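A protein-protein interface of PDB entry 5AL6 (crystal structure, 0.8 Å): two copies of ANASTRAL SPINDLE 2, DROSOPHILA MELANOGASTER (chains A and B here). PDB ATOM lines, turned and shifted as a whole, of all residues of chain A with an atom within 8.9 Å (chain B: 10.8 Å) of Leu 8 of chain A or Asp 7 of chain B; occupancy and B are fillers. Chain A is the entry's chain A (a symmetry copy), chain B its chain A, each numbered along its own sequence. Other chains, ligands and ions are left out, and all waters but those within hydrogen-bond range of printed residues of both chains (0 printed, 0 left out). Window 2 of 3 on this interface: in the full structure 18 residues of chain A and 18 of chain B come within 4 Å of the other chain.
Of chain B, only Asp 7 (3.0 Å) and Leu 11 (3.6 Å) come within 4 Å of Leu 8 of chain A.
Of the printed residues of chain A, Asp 7 of chain B touches Leu 8.
No residue of chain B comes within 4 Å of Ser 6 of chain A.
No residue of chain B comes within 4 Å of Ala 9 of chain A.
Leu 11 of chain A touches just one residue of chain B: Leu 11.
Of the printed residues of chain A, Leu 14 of chain B touches Val 12 (3.997 Å) and Val 15 (3.5 Å).
Of the printed residues of chain B, Val 12 of chain A touches Leu 14.
Of the printed residues of chain B, Val 15 of chain A touches Leu 14 and Val 15.
Of the printed residues of chain A, Leu 11 of chain B touches Leu 8 and Leu 11.
Printed residues of chain A within 4 Å of Val 15 of chain B: Val 15.
Val 12 of chain B touches none of the printed residues of chain A.
Leu 8 of chain B touches none of the printed residues of chain A.
The nearest residue of chain A that does not touch Asp 7 of chain B is Val 12 of chain A (5.0 Å).
Leu 8 of chain A touches Leu 11 of chain B, but with the chains exchanged Leu 11 of chain A does not touch Leu 8 of chain B (6.9 Å).
Leu 11 of chain B touches its own counterpart, Leu 11 of chain A.
Val 12 of chain A touches Leu 14 of chain B, but with the chains exchanged Leu 14 of chain A does not touch Val 12 of chain B (11.7 Å).
Val 15 of chain B touches its own counterpart, Val 15 of chain A.
Positions printed for both chains: 6, 7, 8, 9, 10, 11, 12, 13, 14 and 15.
Among the printed residues, no Asp or Glu carboxylate lies within 4 Å of a Lys or Arg side-chain nitrogen of the other chain.
The side-chain hydroxyl (OG) of Ser 6 of chain B lies within hydrogen-bond range of the side-chain carboxylate (OD1) of Asp 7 of chain B.
Among the printed residues, merely in contact across the chains: Leu 8 of chain A with Asp 7 of chain B (3.0 Å), Val 15 of chain A with Leu 14 of chain B (3.5 Å), Leu 8 of chain A with Leu 11 of chain B (3.6 Å), Leu 11 of chain A with Leu 11 of chain B (3.7 Å), Val 15 of chain A with Val 15 of chain B (3.97 Å) and Val 12 of chain A with Leu 14 of chain B (3.997 Å).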
ATOM      1  N   SER A   6      -3.847  23.460  -7.551  1.00  0.00           N
ATOM      2  CA  SER A   6      -3.171  24.816  -7.783  1.00  0.00           C
ATOM      3  C   SER A   6      -2.208  24.631  -8.955  1.00  0.00           C
ATOM      4  O   SER A   6      -2.524  25.013 -10.104  1.00  0.00           O
ATOM      5  CB  SER A   6      -2.492  25.509  -6.452  1.00  0.00           C
ATOM      6  OG  SER A   6      -1.114  25.154  -6.025  1.00  0.00           O
ATOM      7  N   ASP A   7      -1.074  23.965  -8.768  1.00  0.00           N
ATOM      8  CA  ASP A   7      -0.269  23.511  -9.966  1.00  0.00           C
ATOM      9  C   ASP A   7      -1.069  22.537 -10.908  1.00  0.00           C
ATOM     10  O   ASP A   7      -0.947  22.615 -12.226  1.00  0.00           O
ATOM     11  CB  ASP A   7       1.058  22.794  -9.552  1.00  0.00           C
ATOM     12  CG  ASP A   7       1.861  23.446  -8.479  1.00  0.00           C
ATOM     13  OD1 ASP A   7       1.274  23.896  -7.423  1.00  0.00           O
ATOM     14  OD2 ASP A   7       3.150  23.392  -8.684  1.00  0.00           O
ATOM     15  N   LEU A   8      -1.823  21.649 -10.177  1.00  0.00           N
ATOM     16  CA  LEU A   8      -2.774  20.633 -10.927  1.00  0.00           C
ATOM     17  C   LEU A   8      -3.821  21.445 -11.666  1.00  0.00           C
ATOM     18  O   LEU A   8      -3.977  21.279 -12.873  1.00  0.00           O
ATOM     19  CB  LEU A   8      -3.231  19.702  -9.973  1.00  0.00           C
ATOM     20  CG  LEU A   8      -3.985  18.743 -10.880  1.00  0.00           C
ATOM     21  CD1 LEU A   8      -3.326  17.984 -11.926  1.00  0.00           C
ATOM     22  CD2 LEU A   8      -4.492  17.669  -9.775  1.00  0.00           C
ATOM     23  N   ALA A   9      -4.476  22.385 -10.989  1.00  0.00           N
ATOM     24  CA  ALA A   9      -5.461  23.200 -11.672  1.00  0.00           C
ATOM     25  C   ALA A   9      -4.902  23.955 -12.883  1.00  0.00           C
ATOM     26  O   ALA A   9      -5.546  24.030 -13.925  1.00  0.00           O
ATOM     27  CB  ALA A   9      -6.104  24.181 -10.688  1.00  0.00           C
ATOM     28  N   ALA A  10      -3.710  24.508 -12.752  1.00  0.00           N
ATOM     29  CA  ALA A  10      -3.126  25.256 -13.867  1.00  0.00           C
ATOM     30  C   ALA A  10      -2.837  24.309 -15.054  1.00  0.00           C
ATOM     31  O   ALA A  10      -2.995  24.683 -16.222  1.00  0.00           O
ATOM     32  CB  ALA A  10      -1.855  25.976 -13.426  1.00  0.00           C
ATOM     33  N   LEU A  11      -2.386  23.092 -14.760  1.00  0.00           N
ATOM     34  CA  LEU A  11      -2.145  22.115 -15.814  1.00  0.00           C
ATOM     35  C   LEU A  11      -3.453  21.688 -16.499  1.00  0.00           C
ATOM     36  O   LEU A  11      -3.504  21.551 -17.723  1.00  0.00           O
ATOM     37  CB  LEU A  11      -1.386  20.916 -15.246  1.00  0.00           C
ATOM     38  CG  LEU A  11      -1.106  19.777 -16.225  1.00  0.00           C
ATOM     39  CD1 LEU A  11      -0.398  20.256 -17.496  1.00  0.00           C
ATOM     40  CD2 LEU A  11      -0.318  18.697 -15.508  1.00  0.00           C
ATOM     41  N   VAL A  12      -4.511  21.479 -15.710  1.00  0.00           N
ATOM     42  CA  VAL A  12      -5.794  21.155 -16.313  1.00  0.00           C
ATOM     43  C   VAL A  12      -6.243  22.271 -17.278  1.00  0.00           C
ATOM     44  O   VAL A  12      -6.686  22.009 -18.390  1.00  0.00           O
ATOM     45  CB  VAL A  12      -6.880  20.876 -15.237  1.00  0.00           C
ATOM     46  CG1 VAL A  12      -8.227  20.600 -15.890  1.00  0.00           C
ATOM     47  CG2 VAL A  12      -6.470  19.672 -14.361  1.00  0.00           C
ATOM     48  N   SER A  13      -6.115  23.526 -16.830  1.00  0.00           N
ATOM     49  CA  SER A  13      -6.475  24.633 -17.712  1.00  0.00           C
ATOM     50  C   SER A  13      -5.657  24.631 -19.006  1.00  0.00           C
ATOM     51  O   SER A  13      -6.206  24.855 -20.096  1.00  0.00           O
ATOM     52  CB  SER A  13      -6.266  25.979 -16.977  1.00  0.00           C
ATOM     53  OG  SER A  13      -6.473  27.048 -17.862  1.00  0.00           O
ATOM     54  N   LEU A  14      -4.354  24.381 -18.896  1.00  0.00           N
ATOM     55  CA  LEU A  14      -3.501  24.314 -20.074  1.00  0.00           C
ATOM     56  C   LEU A  14      -3.968  23.210 -21.041  1.00  0.00           C
ATOM     57  O   LEU A  14      -4.051  23.418 -22.248  1.00  0.00           O
ATOM     58  CB  LEU A  14      -2.039  24.088 -19.631  1.00  0.00           C
ATOM     59  CG  LEU A  14      -1.068  23.774 -20.762  1.00  0.00           C
ATOM     60  CD1 LEU A  14      -0.950  24.879 -21.793  1.00  0.00           C
ATOM     61  CD2 LEU A  14       0.314  23.461 -20.168  1.00  0.00           C
ATOM     62  N   VAL A  15      -4.258  22.016 -20.499  1.00  0.00           N
ATOM     63  CA  VAL A  15      -4.725  20.945 -21.375  1.00  0.00           C
ATOM     64  C   VAL A  15      -6.074  21.307 -22.023  1.00  0.00           C
ATOM     65  O   VAL A  15      -6.298  21.001 -23.202  1.00  0.00           O
ATOM     66  CB  VAL A  15      -4.768  19.596 -20.633  1.00  0.00           C
ATOM     67  CG1 VAL A  15      -5.351  18.509 -21.523  1.00  0.00           C
ATOM     68  CG2 VAL A  15      -3.356  19.191 -20.179  1.00  0.00           C
ATOM     69  N   SER B   6      -7.901  11.242  -8.325  1.00  0.00           N
ATOM     70  CA  SER B   6      -9.249  11.971  -8.328  1.00  0.00           C
ATOM     71  C   SER B   6      -9.082  13.198  -9.223  1.00  0.00           C
ATOM     72  O   SER B   6      -9.508  13.191 -10.399  1.00  0.00           O
ATOM     73  CB  SER B   6      -9.884  12.297  -6.843  1.00  0.00           C
ATOM     74  OG  SER B   6      -9.486  13.516  -6.092  1.00  0.00           O
ATOM     75  N   ASP B   7      -8.387  14.239  -8.777  1.00  0.00           N
ATOM     76  CA  ASP B   7      -7.955  15.317  -9.747  1.00  0.00           C
ATOM     77  C   ASP B   7      -7.029  14.771 -10.897  1.00  0.00           C
ATOM     78  O   ASP B   7      -7.148  15.226 -12.138  1.00  0.00           O
ATOM     79  CB  ASP B   7      -7.197  16.485  -9.037  1.00  0.00           C
ATOM     80  CG  ASP B   7      -7.796  16.997  -7.771  1.00  0.00           C
ATOM     81  OD1 ASP B   7      -8.223  16.166  -6.884  1.00  0.00           O
ATOM     82  OD2 ASP B   7      -7.722  18.295  -7.644  1.00  0.00           O
ATOM     83  N   LEU B   8      -6.134  13.846 -10.415  1.00  0.00           N
ATOM     84  CA  LEU B   8      -5.164  13.105 -11.420  1.00  0.00           C
ATOM     85  C   LEU B   8      -6.022  12.290 -12.370  1.00  0.00           C
ATOM     86  O   LEU B   8      -5.899  12.445 -13.582  1.00  0.00           O
ATOM     87  CB  LEU B   8      -4.213  12.408 -10.649  1.00  0.00           C
ATOM     88  CG  LEU B   8      -3.300  11.899 -11.752  1.00  0.00           C
ATOM     89  CD1 LEU B   8      -2.562  12.792 -12.624  1.00  0.00           C
ATOM     90  CD2 LEU B   8      -2.202  11.114 -10.853  1.00  0.00           C
ATOM     91  N   ALA B   9      -6.953  11.496 -11.848  1.00  0.00           N
ATOM     92  CA  ALA B   9      -7.811  10.728 -12.728  1.00  0.00           C
ATOM     93  C   ALA B   9      -8.593  11.586 -13.729  1.00  0.00           C
ATOM     94  O   ALA B   9      -8.716  11.230 -14.896  1.00  0.00           O
ATOM     95  CB  ALA B   9      -8.773   9.867 -11.904  1.00  0.00           C
ATOM     96  N   ALA B  10      -9.116  12.712 -13.278  1.00  0.00           N
ATOM     97  CA  ALA B  10      -9.888  13.571 -14.180  1.00  0.00           C
ATOM     98  C   ALA B  10      -8.974  14.140 -15.289  1.00  0.00           C
ATOM     99  O   ALA B  10      -9.389  14.290 -16.443  1.00  0.00           O
ATOM    100  CB  ALA B  10     -10.565  14.696 -13.403  1.00  0.00           C
ATOM    101  N   LEU B  11      -7.739  14.487 -14.935  1.00  0.00           N
ATOM    102  CA  LEU B  11      -6.792  14.977 -15.928  1.00  0.00           C
ATOM    103  C   LEU B  11      -6.416  13.881 -16.939  1.00  0.00           C
ATOM    104  O   LEU B  11      -6.320  14.142 -18.139  1.00  0.00           O
ATOM    105  CB  LEU B  11      -5.559  15.551 -15.231  1.00  0.00           C
ATOM    106  CG  LEU B  11      -4.447  16.057 -16.148  1.00  0.00           C
ATOM    107  CD1 LEU B  11      -4.952  17.071 -17.178  1.00  0.00           C
ATOM    108  CD2 LEU B  11      -3.328  16.623 -15.295  1.00  0.00           C
ATOM    109  N   VAL B  12      -6.204  12.655 -16.452  1.00  0.00           N
ATOM    110  CA  VAL B  12      -5.926  11.564 -17.374  1.00  0.00           C
ATOM    111  C   VAL B  12      -7.083  11.389 -18.379  1.00  0.00           C
ATOM    112  O   VAL B  12      -6.867  11.241 -19.576  1.00  0.00           O
ATOM    113  CB  VAL B  12      -5.636  10.236 -16.620  1.00  0.00           C
ATOM    114  CG1 VAL B  12      -5.410   9.097 -17.604  1.00  0.00           C
ATOM    115  CG2 VAL B  12      -4.395  10.395 -15.714  1.00  0.00           C
ATOM    116  N   SER B  13      -8.320  11.415 -17.867  1.00  0.00           N
ATOM    117  CA  SER B  13      -9.462  11.305 -18.769  1.00  0.00           C
ATOM    118  C   SER B  13      -9.486  12.426 -19.812  1.00  0.00           C
ATOM    119  O   SER B  13      -9.756  12.175 -20.997  1.00  0.00           O
ATOM    120  CB  SER B  13     -10.779  11.336 -17.956  1.00  0.00           C
ATOM    121  OG  SER B  13     -11.880  11.374 -18.825  1.00  0.00           O
ATOM    122  N   LEU B  14      -9.204  13.654 -19.384  1.00  0.00           N
ATOM    123  CA  LEU B  14      -9.158  14.778 -20.308  1.00  0.00           C
ATOM    124  C   LEU B  14      -8.096  14.560 -21.402  1.00  0.00           C
ATOM    125  O   LEU B  14      -8.345  14.789 -22.582  1.00  0.00           O
ATOM    126  CB  LEU B  14      -8.886  16.076 -19.517  1.00  0.00           C
ATOM    127  CG  LEU B  14      -8.588  17.299 -20.374  1.00  0.00           C
ATOM    128  CD1 LEU B  14      -9.724  17.690 -21.300  1.00  0.00           C
ATOM    129  CD2 LEU B  14      -8.227  18.480 -19.461  1.00  0.00           C
ATOM    130  N   VAL B  15      -6.891  14.127 -20.997  1.00  0.00           N
ATOM    131  CA  VAL B  15      -5.860  13.885 -22.002  1.00  0.00           C
ATOM    132  C   VAL B  15      -6.271  12.751 -22.958  1.00  0.00           C
ATOM    133  O   VAL B  15      -6.009  12.830 -24.165  1.00  0.00           O
ATOM    134  CB  VAL B  15      -4.489  13.637 -21.346  1.00  0.00           C
ATOM    135  CG1 VAL B  15      -3.444  13.288 -22.395  1.00  0.00           C
ATOM    136  CG2 VAL B  15      -4.039  14.882 -20.563  1.00  0.00           C
